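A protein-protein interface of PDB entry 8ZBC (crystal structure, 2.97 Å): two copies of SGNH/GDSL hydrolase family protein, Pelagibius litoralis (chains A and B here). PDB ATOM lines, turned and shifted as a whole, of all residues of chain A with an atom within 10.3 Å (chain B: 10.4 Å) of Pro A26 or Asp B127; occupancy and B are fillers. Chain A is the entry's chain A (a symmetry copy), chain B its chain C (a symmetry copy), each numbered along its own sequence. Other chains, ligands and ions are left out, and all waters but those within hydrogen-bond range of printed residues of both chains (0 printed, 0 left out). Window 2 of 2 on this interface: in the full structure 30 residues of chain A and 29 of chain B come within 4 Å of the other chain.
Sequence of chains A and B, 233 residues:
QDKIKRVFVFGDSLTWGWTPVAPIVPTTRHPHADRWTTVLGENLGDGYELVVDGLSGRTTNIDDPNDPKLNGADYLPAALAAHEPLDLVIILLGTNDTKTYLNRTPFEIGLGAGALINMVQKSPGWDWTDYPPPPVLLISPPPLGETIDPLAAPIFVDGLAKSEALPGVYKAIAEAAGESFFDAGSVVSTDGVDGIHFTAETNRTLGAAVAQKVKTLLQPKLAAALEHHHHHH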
ATOM      1  N   TRP A  16     -30.613  16.262   8.069  1.00  0.00           N
ATOM      2  CA  TRP A  16     -31.676  17.210   7.736  1.00  0.00           C
ATOM      3  C   TRP A  16     -31.728  17.432   6.236  1.00  0.00           C
ATOM      4  O   TRP A  16     -32.795  17.432   5.635  1.00  0.00           O
ATOM      5  CB  TRP A  16     -31.424  18.559   8.432  1.00  0.00           C
ATOM      6  CG  TRP A  16     -32.447  19.652   8.144  1.00  0.00           C
ATOM      7  CD1 TRP A  16     -33.738  19.699   8.581  1.00  0.00           C
ATOM      8  CD2 TRP A  16     -32.240  20.848   7.378  1.00  0.00           C
ATOM      9  NE1 TRP A  16     -34.360  20.835   8.115  1.00  0.00           N
ATOM     10  CE2 TRP A  16     -33.458  21.562   7.382  1.00  0.00           C
ATOM     11  CE3 TRP A  16     -31.153  21.372   6.670  1.00  0.00           C
ATOM     12  CZ2 TRP A  16     -33.610  22.782   6.718  1.00  0.00           C
ATOM     13  CZ3 TRP A  16     -31.316  22.577   5.996  1.00  0.00           C
ATOM     14  CH2 TRP A  16     -32.530  23.266   6.025  1.00  0.00           C
ATOM     15  N   GLY A  17     -30.560  17.633   5.640  1.00  0.00           N
ATOM     16  CA  GLY A  17     -30.430  17.859   4.195  1.00  0.00           C
ATOM     17  C   GLY A  17     -29.904  19.233   3.854  1.00  0.00           C
ATOM     18  O   GLY A  17     -30.491  19.937   3.045  1.00  0.00           O
ATOM     19  N   TRP A  18     -28.791  19.613   4.460  1.00  0.00           N
ATOM     20  CA  TRP A  18     -28.168  20.902   4.184  1.00  0.00           C
ATOM     21  C   TRP A  18     -27.623  20.929   2.776  1.00  0.00           C
ATOM     22  O   TRP A  18     -26.783  20.101   2.428  1.00  0.00           O
ATOM     23  CB  TRP A  18     -27.060  21.176   5.187  1.00  0.00           C
ATOM     24  CG  TRP A  18     -26.405  22.536   5.095  1.00  0.00           C
ATOM     25  CD1 TRP A  18     -25.734  23.059   4.021  1.00  0.00           C
ATOM     26  CD2 TRP A  18     -26.308  23.508   6.138  1.00  0.00           C
ATOM     27  NE1 TRP A  18     -25.258  24.307   4.332  1.00  0.00           N
ATOM     28  CE2 TRP A  18     -25.597  24.601   5.631  1.00  0.00           C
ATOM     29  CE3 TRP A  18     -26.757  23.559   7.459  1.00  0.00           C
ATOM     30  CZ2 TRP A  18     -25.330  25.737   6.404  1.00  0.00           C
ATOM     31  CZ3 TRP A  18     -26.485  24.706   8.222  1.00  0.00           C
ATOM     32  CH2 TRP A  18     -25.785  25.763   7.688  1.00  0.00           C
ATOM     33  N   THR A  19     -28.101  21.886   1.977  1.00  0.00           N
ATOM     34  CA  THR A  19     -27.596  22.092   0.623  1.00  0.00           C
ATOM     35  C   THR A  19     -26.342  22.975   0.708  1.00  0.00           C
ATOM     36  O   THR A  19     -26.441  24.116   1.139  1.00  0.00           O
ATOM     37  CB  THR A  19     -28.640  22.775  -0.286  1.00  0.00           C
ATOM     38  OG1 THR A  19     -29.823  21.982  -0.361  1.00  0.00           O
ATOM     39  CG2 THR A  19     -28.097  22.935  -1.682  1.00  0.00           C
ATOM     40  N   PRO A  20     -25.159  22.444   0.315  1.00  0.00           N
ATOM     41  CA  PRO A  20     -23.954  23.253   0.331  1.00  0.00           C
ATOM     42  C   PRO A  20     -24.000  24.399  -0.686  1.00  0.00           C
ATOM     43  O   PRO A  20     -24.384  24.183  -1.836  1.00  0.00           O
ATOM     44  CB  PRO A  20     -22.837  22.256  -0.030  1.00  0.00           C
ATOM     45  CG  PRO A  20     -23.488  21.088  -0.650  1.00  0.00           C
ATOM     46  CD  PRO A  20     -24.874  21.052  -0.087  1.00  0.00           C
ATOM     47  N   VAL A  21     -23.629  25.601  -0.236  1.00  0.00           N
ATOM     48  CA  VAL A  21     -23.756  26.810  -1.047  1.00  0.00           C
ATOM     49  C   VAL A  21     -22.702  27.849  -0.680  1.00  0.00           C
ATOM     50  O   VAL A  21     -21.980  27.707   0.310  1.00  0.00           O
ATOM     51  CB  VAL A  21     -25.152  27.459  -0.873  1.00  0.00           C
ATOM     52  CG1 VAL A  21     -26.220  26.648  -1.575  1.00  0.00           C
ATOM     53  CG2 VAL A  21     -25.506  27.617   0.603  1.00  0.00           C
ATOM     54  N   ALA A  22     -22.618  28.896  -1.493  1.00  0.00           N
ATOM     55  CA  ALA A  22     -21.717  30.001  -1.252  1.00  0.00           C
ATOM     56  C   ALA A  22     -22.503  31.313  -1.369  1.00  0.00           C
ATOM     57  O   ALA A  22     -23.164  31.542  -2.382  1.00  0.00           O
ATOM     58  CB  ALA A  22     -20.595  29.962  -2.266  1.00  0.00           C
ATOM     59  N   PRO A  23     -22.485  32.155  -0.333  1.00  0.00           N
ATOM     60  CA  PRO A  23     -21.825  31.859   0.940  1.00  0.00           C
ATOM     61  C   PRO A  23     -22.537  30.728   1.718  1.00  0.00           C
ATOM     62  O   PRO A  23     -23.694  30.397   1.422  1.00  0.00           O
ATOM     63  CB  PRO A  23     -21.888  33.202   1.681  1.00  0.00           C
ATOM     64  CG  PRO A  23     -23.041  33.939   1.059  1.00  0.00           C
ATOM     65  CD  PRO A  23     -23.523  33.182  -0.158  1.00  0.00           C
ATOM     66  N   ILE A  24     -21.826  30.164   2.695  1.00  0.00           N
ATOM     67  CA  ILE A  24     -22.265  28.952   3.448  1.00  0.00           C
ATOM     68  C   ILE A  24     -23.706  29.035   3.968  1.00  0.00           C
ATOM     69  O   ILE A  24     -24.417  28.037   3.936  1.00  0.00           O
ATOM     70  CB  ILE A  24     -21.306  28.609   4.618  1.00  0.00           C
ATOM     71  CG1 ILE A  24     -21.705  27.333   5.311  1.00  0.00           C
ATOM     72  CG2 ILE A  24     -21.217  29.734   5.642  1.00  0.00           C
ATOM     73  CD1 ILE A  24     -20.660  26.796   6.301  1.00  0.00           C
ATOM     74  N   VAL A  25     -24.100  30.230   4.419  1.00  0.00           N
ATOM     75  CA  VAL A  25     -25.438  30.540   4.897  1.00  0.00           C
ATOM     76  C   VAL A  25     -25.977  31.797   4.192  1.00  0.00           C
ATOM     77  O   VAL A  25     -25.197  32.662   3.821  1.00  0.00           O
ATOM     78  CB  VAL A  25     -25.504  30.760   6.424  1.00  0.00           C
ATOM     79  CG1 VAL A  25     -25.073  29.504   7.157  1.00  0.00           C
ATOM     80  CG2 VAL A  25     -24.669  31.968   6.853  1.00  0.00           C
ATOM     81  N   PRO A  26     -27.293  31.900   3.994  1.00  0.00           N
ATOM     82  CA  PRO A  26     -28.267  30.861   4.323  1.00  0.00           C
ATOM     83  C   PRO A  26     -28.322  29.729   3.285  1.00  0.00           C
ATOM     84  O   PRO A  26     -27.935  29.913   2.128  1.00  0.00           O
ATOM     85  CB  PRO A  26     -29.583  31.629   4.294  1.00  0.00           C
ATOM     86  CG  PRO A  26     -29.360  32.744   3.297  1.00  0.00           C
ATOM     87  CD  PRO A  26     -27.885  33.025   3.246  1.00  0.00           C
ATOM     88  N   THR A  27     -28.802  28.571   3.730  1.00  0.00           N
ATOM     89  CA  THR A  27     -29.007  27.404   2.873  1.00  0.00           C
ATOM     90  C   THR A  27     -30.500  27.129   2.736  1.00  0.00           C
ATOM     91  O   THR A  27     -31.343  27.780   3.372  1.00  0.00           O
ATOM     92  CB  THR A  27     -28.292  26.143   3.429  1.00  0.00           C
ATOM     93  OG1 THR A  27     -28.519  25.011   2.565  1.00  0.00           O
ATOM     94  CG2 THR A  27     -28.782  25.790   4.834  1.00  0.00           C
ATOM     95  N   THR A  28     -30.825  26.175   1.878  1.00  0.00           N
ATOM     96  CA  THR A  28     -32.178  25.650   1.783  1.00  0.00           C
ATOM     97  C   THR A  28     -32.063  24.131   1.849  1.00  0.00           C
ATOM     98  O   THR A  28     -30.991  23.564   1.575  1.00  0.00           O
ATOM     99  CB  THR A  28     -32.889  26.077   0.480  1.00  0.00           C
ATOM    100  OG1 THR A  28     -32.336  25.357  -0.617  1.00  0.00           O
ATOM    101  CG2 THR A  28     -32.756  27.580   0.219  1.00  0.00           C
ATOM    102  N   ARG A  29     -33.158  23.480   2.215  1.00  0.00           N
ATOM    103  CA  ARG A  29     -33.146  22.034   2.442  1.00  0.00           C
ATOM    104  C   ARG A  29     -33.095  21.282   1.129  1.00  0.00           C
ATOM    105  O   ARG A  29     -33.853  21.588   0.214  1.00  0.00           O
ATOM    106  CB  ARG A  29     -34.393  21.603   3.224  1.00  0.00           C
ATOM    107  CG  ARG A  29     -34.099  20.553   4.284  1.00  0.00           C
ATOM    108  CD  ARG A  29     -35.072  19.400   4.271  1.00  0.00           C
ATOM    109  NE  ARG A  29     -36.092  19.444   5.323  1.00  0.00           N
ATOM    110  CZ  ARG A  29     -36.250  18.542   6.291  1.00  0.00           C
ATOM    111  NH1 ARG A  29     -35.431  17.513   6.414  1.00  0.00           N
ATOM    112  NH2 ARG A  29     -37.238  18.675   7.157  1.00  0.00           N
ATOM    113  N   SER A  56     -29.758  20.622  12.246  1.00  0.00           N
ATOM    114  CA  SER A  56     -28.572  21.413  11.947  1.00  0.00           C
ATOM    115  C   SER A  56     -27.924  21.828  13.253  1.00  0.00           C
ATOM    116  O   SER A  56     -28.589  22.303  14.158  1.00  0.00           O
ATOM    117  CB  SER A  56     -28.921  22.653  11.103  1.00  0.00           C
ATOM    118  OG  SER A  56     -29.691  22.327   9.939  1.00  0.00           O
ATOM    119  N   ASN A  66     -23.687  28.595  22.249  1.00  0.00           N
ATOM    120  CA  ASN A  66     -24.371  29.504  21.324  1.00  0.00           C
ATOM    121  C   ASN A  66     -25.839  29.200  21.069  1.00  0.00           C
ATOM    122  O   ASN A  66     -26.550  30.026  20.537  1.00  0.00           O
ATOM    123  CB  ASN A  66     -23.646  29.522  19.983  1.00  0.00           C
ATOM    124  CG  ASN A  66     -22.214  29.973  20.112  1.00  0.00           C
ATOM    125  OD1 ASN A  66     -21.956  31.144  20.331  1.00  0.00           O
ATOM    126  ND2 ASN A  66     -21.273  29.042  19.975  1.00  0.00           N
ATOM    127  N   ASP A  67     -26.291  28.007  21.430  1.00  0.00           N
ATOM    128  CA  ASP A  67     -27.662  27.571  21.127  1.00  0.00           C
ATOM    129  C   ASP A  67     -28.034  26.387  22.024  1.00  0.00           C
ATOM    130  O   ASP A  67     -27.460  25.286  21.906  1.00  0.00           O
ATOM    131  CB  ASP A  67     -27.789  27.185  19.654  1.00  0.00           C
ATOM    132  CG  ASP A  67     -29.241  26.969  19.229  1.00  0.00           C
ATOM    133  OD1 ASP A  67     -30.155  26.851  20.099  1.00  0.00           O
ATOM    134  OD2 ASP A  67     -29.458  26.922  18.009  1.00  0.00           O
ATOM    135  N   LYS A  69     -30.422  24.295  22.051  1.00  0.00           N
ATOM    136  CA  LYS A  69     -31.166  23.136  21.530  1.00  0.00           C
ATOM    137  C   LYS A  69     -30.357  22.089  20.758  1.00  0.00           C
ATOM    138  O   LYS A  69     -30.945  21.206  20.141  1.00  0.00           O
ATOM    139  CB  LYS A  69     -32.330  23.619  20.650  1.00  0.00           C
ATOM    140  CG  LYS A  69     -31.946  24.186  19.275  1.00  0.00           C
ATOM    141  CD  LYS A  69     -33.160  24.703  18.536  1.00  0.00           C
ATOM    142  CE  LYS A  69     -32.786  25.278  17.175  1.00  0.00           C
ATOM    143  NZ  LYS A  69     -32.217  26.662  17.240  1.00  0.00           N
ATOM    144  N   ASP A 149     -15.668  27.068   4.170  1.00  0.00           N
ATOM    145  CA  ASP A 149     -16.116  28.426   3.930  1.00  0.00           C
ATOM    146  C   ASP A 149     -15.491  29.344   4.983  1.00  0.00           C
ATOM    147  O   ASP A 149     -15.569  29.045   6.180  1.00  0.00           O
ATOM    148  CB  ASP A 149     -17.633  28.488   3.984  1.00  0.00           C
ATOM    149  CG  ASP A 149     -18.189  29.803   3.483  1.00  0.00           C
ATOM    150  OD1 ASP A 149     -17.797  30.862   4.004  1.00  0.00           O
ATOM    151  OD2 ASP A 149     -19.059  29.776   2.596  1.00  0.00           O
ATOM    152  N   LEU A 151     -16.361  31.959   6.483  1.00  0.00           N
ATOM    153  CA  LEU A 151     -17.251  32.293   7.606  1.00  0.00           C
ATOM    154  C   LEU A 151     -17.217  31.227   8.716  1.00  0.00           C
ATOM    155  O   LEU A 151     -17.272  31.555   9.894  1.00  0.00           O
ATOM    156  CB  LEU A 151     -18.688  32.478   7.137  1.00  0.00           C
ATOM    157  CG  LEU A 151     -18.999  33.810   6.435  1.00  0.00           C
ATOM    158  CD1 LEU A 151     -19.534  33.618   5.012  1.00  0.00           C
ATOM    159  CD2 LEU A 151     -19.962  34.642   7.271  1.00  0.00           C
ATOM    160  N   ALA A 152     -17.109  29.958   8.326  1.00  0.00           N
ATOM    161  CA  ALA A 152     -17.145  28.842   9.267  1.00  0.00           C
ATOM    162  C   ALA A 152     -15.758  28.329   9.694  1.00  0.00           C
ATOM    163  O   ALA A 152     -15.634  27.699  10.734  1.00  0.00           O
ATOM    164  CB  ALA A 152     -17.965  27.709   8.662  1.00  0.00           C
ATOM    165  N   ILE A 155     -14.301  28.381  13.370  1.00  0.00           N
ATOM    166  CA  ILE A 155     -15.028  27.484  14.255  1.00  0.00           C
ATOM    167  C   ILE A 155     -14.661  25.998  14.048  1.00  0.00           C
ATOM    168  O   ILE A 155     -15.037  25.157  14.863  1.00  0.00           O
ATOM    169  CB  ILE A 155     -16.549  27.824  14.106  1.00  0.00           C
ATOM    170  CG1 ILE A 155     -16.931  28.840  15.189  1.00  0.00           C
ATOM    171  CG2 ILE A 155     -17.483  26.616  14.077  1.00  0.00           C
ATOM    172  CD1 ILE A 155     -18.294  29.492  14.977  1.00  0.00           C
ATOM    173  N   VAL A 193     -19.433  22.383  -1.477  1.00  0.00           N
ATOM    174  CA  VAL A 193     -18.609  23.564  -1.705  1.00  0.00           C
ATOM    175  C   VAL A 193     -18.162  24.264  -0.414  1.00  0.00           C
ATOM    176  O   VAL A 193     -17.090  24.868  -0.390  1.00  0.00           O
ATOM    177  CB  VAL A 193     -19.295  24.570  -2.656  1.00  0.00           C
ATOM    178  CG1 VAL A 193     -20.457  25.295  -1.954  1.00  0.00           C
ATOM    179  CG2 VAL A 193     -18.259  25.539  -3.223  1.00  0.00           C
ATOM    180  N   ASP A 194     -18.956  24.165   0.657  1.00  0.00           N
ATOM    181  CA  ASP A 194     -18.613  24.848   1.921  1.00  0.00           C
ATOM    182  C   ASP A 194     -17.675  24.040   2.815  1.00  0.00           C
ATOM    183  O   ASP A 194     -17.307  24.498   3.902  1.00  0.00           O
ATOM    184  CB  ASP A 194     -19.877  25.279   2.703  1.00  0.00           C
ATOM    185  CG  ASP A 194     -20.816  24.106   3.053  1.00  0.00           C
ATOM    186  OD1 ASP A 194     -20.390  22.926   2.956  1.00  0.00           O
ATOM    187  OD2 ASP A 194     -21.972  24.377   3.423  1.00  0.00           O
ATOM    188  N   HIS A 197     -20.833  20.064   4.226  1.00  0.00           N
ATOM    189  CA  HIS A 197     -22.054  19.332   3.886  1.00  0.00           C
ATOM    190  C   HIS A 197     -21.931  18.605   2.554  1.00  0.00           C
ATOM    191  O   HIS A 197     -20.894  18.668   1.889  1.00  0.00           O
ATOM    192  CB  HIS A 197     -23.226  20.292   3.887  1.00  0.00           C
ATOM    193  CG  HIS A 197     -23.313  21.091   5.143  1.00  0.00           C
ATOM    194  ND1 HIS A 197     -22.881  22.394   5.232  1.00  0.00           N
ATOM    195  CD2 HIS A 197     -23.712  20.743   6.386  1.00  0.00           C
ATOM    196  CE1 HIS A 197     -23.042  22.827   6.470  1.00  0.00           C
ATOM    197  NE2 HIS A 197     -23.544  21.843   7.190  1.00  0.00           N
ATOM    198  N   GLU B  84     -38.031  22.017   9.757  1.00  0.00           N
ATOM    199  CA  GLU B  84     -38.154  23.193   8.897  1.00  0.00           C
ATOM    200  C   GLU B  84     -37.861  22.796   7.429  1.00  0.00           C
ATOM    201  O   GLU B  84     -36.908  22.045   7.174  1.00  0.00           O
ATOM    202  CB  GLU B  84     -37.177  24.285   9.353  1.00  0.00           C
ATOM    203  CG  GLU B  84     -37.366  25.624   8.649  1.00  0.00           C
ATOM    204  CD  GLU B  84     -36.357  26.678   9.031  1.00  0.00           C
ATOM    205  OE1 GLU B  84     -36.808  27.833   9.226  1.00  0.00           O
ATOM    206  OE2 GLU B  84     -35.132  26.360   9.139  1.00  0.00           O
ATOM    207  N   LYS B 122     -40.617  32.120  17.373  1.00  0.00           N
ATOM    208  CA  LYS B 122     -39.193  32.450  17.319  1.00  0.00           C
ATOM    209  C   LYS B 122     -38.383  31.341  16.651  1.00  0.00           C
ATOM    210  O   LYS B 122     -37.176  31.340  16.724  1.00  0.00           O
ATOM    211  CB  LYS B 122     -38.675  32.686  18.739  1.00  0.00           C
ATOM    212  CG  LYS B 122     -39.466  33.741  19.499  1.00  0.00           C
ATOM    213  CD  LYS B 122     -39.015  33.866  20.936  1.00  0.00           C
ATOM    214  CE  LYS B 122     -37.743  34.682  21.050  1.00  0.00           C
ATOM    215  NZ  LYS B 122     -36.950  34.290  22.249  1.00  0.00           N
ATOM    216  N   SER B 123     -39.068  30.433  15.963  1.00  0.00           N
ATOM    217  CA  SER B 123     -38.484  29.210  15.399  1.00  0.00           C
ATOM    218  C   SER B 123     -37.458  29.525  14.331  1.00  0.00           C
ATOM    219  O   SER B 123     -37.594  30.531  13.618  1.00  0.00           O
ATOM    220  CB  SER B 123     -39.573  28.349  14.777  1.00  0.00           C
ATOM    221  OG  SER B 123     -39.262  27.009  14.926  1.00  0.00           O
ATOM    222  N   PRO B 124     -36.587  28.546  14.042  1.00  0.00           N
ATOM    223  CA  PRO B 124     -35.133  28.418  14.204  1.00  0.00           C
ATOM    224  C   PRO B 124     -34.563  29.664  14.830  1.00  0.00           C
ATOM    225  O   PRO B 124     -35.019  30.758  14.519  1.00  0.00           O
ATOM    226  CB  PRO B 124     -34.645  28.260  12.766  1.00  0.00           C
ATOM    227  CG  PRO B 124     -35.704  28.836  11.934  1.00  0.00           C
ATOM    228  CD  PRO B 124     -36.906  28.261  12.626  1.00  0.00           C
ATOM    229  N   GLY B 125     -33.573  29.556  15.679  1.00  0.00           N
ATOM    230  CA  GLY B 125     -33.071  30.802  16.249  1.00  0.00           C
ATOM    231  C   GLY B 125     -31.923  31.399  15.469  1.00  0.00           C
ATOM    232  O   GLY B 125     -30.971  31.849  16.078  1.00  0.00           O
ATOM    233  N   TRP B 126     -31.964  31.388  14.136  1.00  0.00           N
ATOM    234  CA  TRP B 126     -30.715  31.546  13.379  1.00  0.00           C
ATOM    235  C   TRP B 126     -30.743  32.074  11.938  1.00  0.00           C
ATOM    236  O   TRP B 126     -31.766  32.057  11.253  1.00  0.00           O
ATOM    237  CB  TRP B 126     -29.936  30.220  13.421  1.00  0.00           C
ATOM    238  CG  TRP B 126     -30.607  29.008  12.760  1.00  0.00           C
ATOM    239  CD1 TRP B 126     -31.336  28.985  11.607  1.00  0.00           C
ATOM    240  CD2 TRP B 126     -30.517  27.644  13.202  1.00  0.00           C
ATOM    241  NE1 TRP B 126     -31.713  27.700  11.313  1.00  0.00           N
ATOM    242  CE2 TRP B 126     -31.214  26.854  12.267  1.00  0.00           C
ATOM    243  CE3 TRP B 126     -29.899  27.012  14.295  1.00  0.00           C
ATOM    244  CZ2 TRP B 126     -31.356  25.471  12.412  1.00  0.00           C
ATOM    245  CZ3 TRP B 126     -30.019  25.630  14.419  1.00  0.00           C
ATOM    246  CH2 TRP B 126     -30.747  24.880  13.486  1.00  0.00           C
ATOM    247  N   ASP B 127     -29.581  32.543  11.507  1.00  0.00           N
ATOM    248  CA  ASP B 127     -29.315  32.960  10.121  1.00  0.00           C
ATOM    249  C   ASP B 127     -28.981  31.794   9.174  1.00  0.00           C
ATOM    250  O   ASP B 127     -28.809  32.024   7.982  1.00  0.00           O
ATOM    251  CB  ASP B 127     -28.193  34.027  10.067  1.00  0.00           C
ATOM    252  CG  ASP B 127     -26.829  33.540  10.675  1.00  0.00           C
ATOM    253  OD1 ASP B 127     -26.829  32.526  11.411  1.00  0.00           O
ATOM    254  OD2 ASP B 127     -25.771  34.152  10.407  1.00  0.00           O
ATOM    255  N   TRP B 128     -28.878  30.565   9.683  1.00  0.00           N
ATOM    256  CA  TRP B 128     -28.444  29.423   8.863  1.00  0.00           C
ATOM    257  C   TRP B 128     -29.438  29.077   7.747  1.00  0.00           C
ATOM    258  O   TRP B 128     -29.048  28.566   6.703  1.00  0.00           O
ATOM    259  CB  TRP B 128     -28.191  28.179   9.717  1.00  0.00           C
ATOM    260  CG  TRP B 128     -27.101  28.339  10.755  1.00  0.00           C
ATOM    261  CD1 TRP B 128     -26.241  29.378  10.874  1.00  0.00           C
ATOM    262  CD2 TRP B 128     -26.744  27.408  11.799  1.00  0.00           C
ATOM    263  NE1 TRP B 128     -25.397  29.178  11.935  1.00  0.00           N
ATOM    264  CE2 TRP B 128     -25.689  27.984  12.527  1.00  0.00           C
ATOM    265  CE3 TRP B 128     -27.241  26.165  12.209  1.00  0.00           C
ATOM    266  CZ2 TRP B 128     -25.093  27.350  13.624  1.00  0.00           C
ATOM    267  CZ3 TRP B 128     -26.642  25.533  13.295  1.00  0.00           C
ATOM    268  CH2 TRP B 128     -25.590  26.135  13.998  1.00  0.00           C
ATOM    269  N   THR B 129     -30.711  29.357   7.983  1.00  0.00           N
ATOM    270  CA  THR B 129     -31.769  29.250   6.992  1.00  0.00           C
ATOM    271  C   THR B 129     -32.561  30.530   7.113  1.00  0.00           C
ATOM    272  O   THR B 129     -32.494  31.182   8.173  1.00  0.00           O
ATOM    273  CB  THR B 129     -32.735  28.051   7.288  1.00  0.00           C
ATOM    274  OG1 THR B 129     -33.369  28.205   8.578  1.00  0.00           O
ATOM    275  CG2 THR B 129     -31.977  26.734   7.270  1.00  0.00           C
ATOM    276  N   ASP B 130     -33.306  30.920   6.078  1.00  0.00           N
ATOM    277  CA  ASP B 130     -34.376  31.884   6.363  1.00  0.00           C
ATOM    278  C   ASP B 130     -35.652  31.602   5.613  1.00  0.00           C
ATOM    279  O   ASP B 130     -35.946  32.168   4.579  1.00  0.00           O
ATOM    280  CB  ASP B 130     -33.921  33.400   6.383  1.00  0.00           C
ATOM    281  CG  ASP B 130     -34.209  34.140   5.116  1.00  0.00           C
ATOM    282  OD1 ASP B 130     -33.619  33.809   4.081  1.00  0.00           O
ATOM    283  OD2 ASP B 130     -34.991  35.101   5.168  1.00  0.00           O
ATOM    284  N   TYR B 131     -36.384  30.658   6.192  1.00  0.00           N
ATOM    285  CA  TYR B 131     -37.794  30.446   5.928  1.00  0.00           C
ATOM    286  C   TYR B 131     -38.544  31.211   7.023  1.00  0.00           C
ATOM    287  O   TYR B 131     -38.009  31.465   8.106  1.00  0.00           O
ATOM    288  CB  TYR B 131     -38.111  28.970   6.057  1.00  0.00           C
ATOM    289  CG  TYR B 131     -37.358  28.033   5.127  1.00  0.00           C
ATOM    290  CD1 TYR B 131     -37.824  27.755   3.848  1.00  0.00           C
ATOM    291  CD2 TYR B 131     -36.202  27.378   5.551  1.00  0.00           C
ATOM    292  CE1 TYR B 131     -37.141  26.884   3.006  1.00  0.00           C
ATOM    293  CE2 TYR B 131     -35.536  26.488   4.724  1.00  0.00           C
ATOM    294  CZ  TYR B 131     -36.003  26.253   3.450  1.00  0.00           C
ATOM    295  OH  TYR B 131     -35.363  25.369   2.621  1.00  0.00           O
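The backbone carbonyl oxygen of Trp B128 is in hydrogen-bond range of the backbone NH of Thr A27 (3.0 Å). NE of Arg A29 lies within hydrogen-bond range of O of Glu B84 (3.3 Å). The side-chain hydroxyl of Tyr B131 sits at hydrogen-bond distance from the backbone NH of Arg A29 (2.9 Å). The backbone carbonyl oxygen (O) of Glu B84 is in hydrogen-bond range of the indole nitrogen (NE1) of Trp A16 (3.0 Å).
OD2 of Asp A67 lies within salt-bridge range of NZ of Lys A69, 2.9 Å away. NH1 of Arg A29 lies within hydrogen-bond range of O of Trp A16, 2.7 Å away. OG1 of Thr A27 sits at hydrogen-bond distance from O of Thr A19, at 2.7 Å. The side-chain hydroxyl (OG1) of Thr A19 sits at hydrogen-bond distance from the backbone carbonyl oxygen (O) of Thr A28, 2.8 Å away. The side-chain hydroxyl (OG1) of Thr B129 lies within hydrogen-bond range of the side-chain carboxylate (OE2) of Glu B84. The indole nitrogen (NE1) of Trp B126 sits at hydrogen-bond distance from the side-chain hydroxyl (OG1) of Thr B129, 3.2 Å away.
Thr B129 touches Trp A16. Val A25 touches Asp B127. Val A25 touches Trp B128 (CG1 to CA, 3.8 Å). CB of Pro A26 touches O of Asp B127 (3.8 Å). CA of Pro A26 touches O of Trp B128 (3.4 Å). Thr A27 touches Thr B129 (O to CA, 3.9 Å). Thr A28 touches Tyr B131. CZ3 of Trp B128 touches O of Ser A56, at 3.9 Å. OD2 of Asp A67 touches CE3 of Trp B126, 3.7 Å away. Gly B125 touches Lys A69.
Of the printed residues of chain B, Trp A16 touches Glu B84 and Thr B129. Ile A24 touches none of the printed residues of chain B. Pro A26 touches just these residues of chain B: Asp B127 and Trp B128. Thr A27 touches just these residues of chain B: Trp B128 (3.0 Å) and Thr B129 (3.9 Å). Printed residues of chain B within 4 Å of Lys A69: Gly B125 (3.6 Å) and Trp B126 (3.7 Å). Pro B124 touches none of the printed residues of chain A. Asp B127 touches just these residues of chain A: Val A25 (3.9 Å) and Pro A26 (3.8 Å). The nearest printed residue of chain B that does not touch Pro A26 is Asp B130 (4.2 Å). The nearest printed residue of chain B that does not touch Arg A29 is Thr B129 (6.1 Å).
Hydrophobic or aromatic side chains of chain B that line the printed part of chain A: Trp B126, Trp B128 and Tyr B131.
No position is printed for both chains. Of the 17 pairs that touch across the chains among the printed residues, none has its exchanged pair printed and touching as well.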
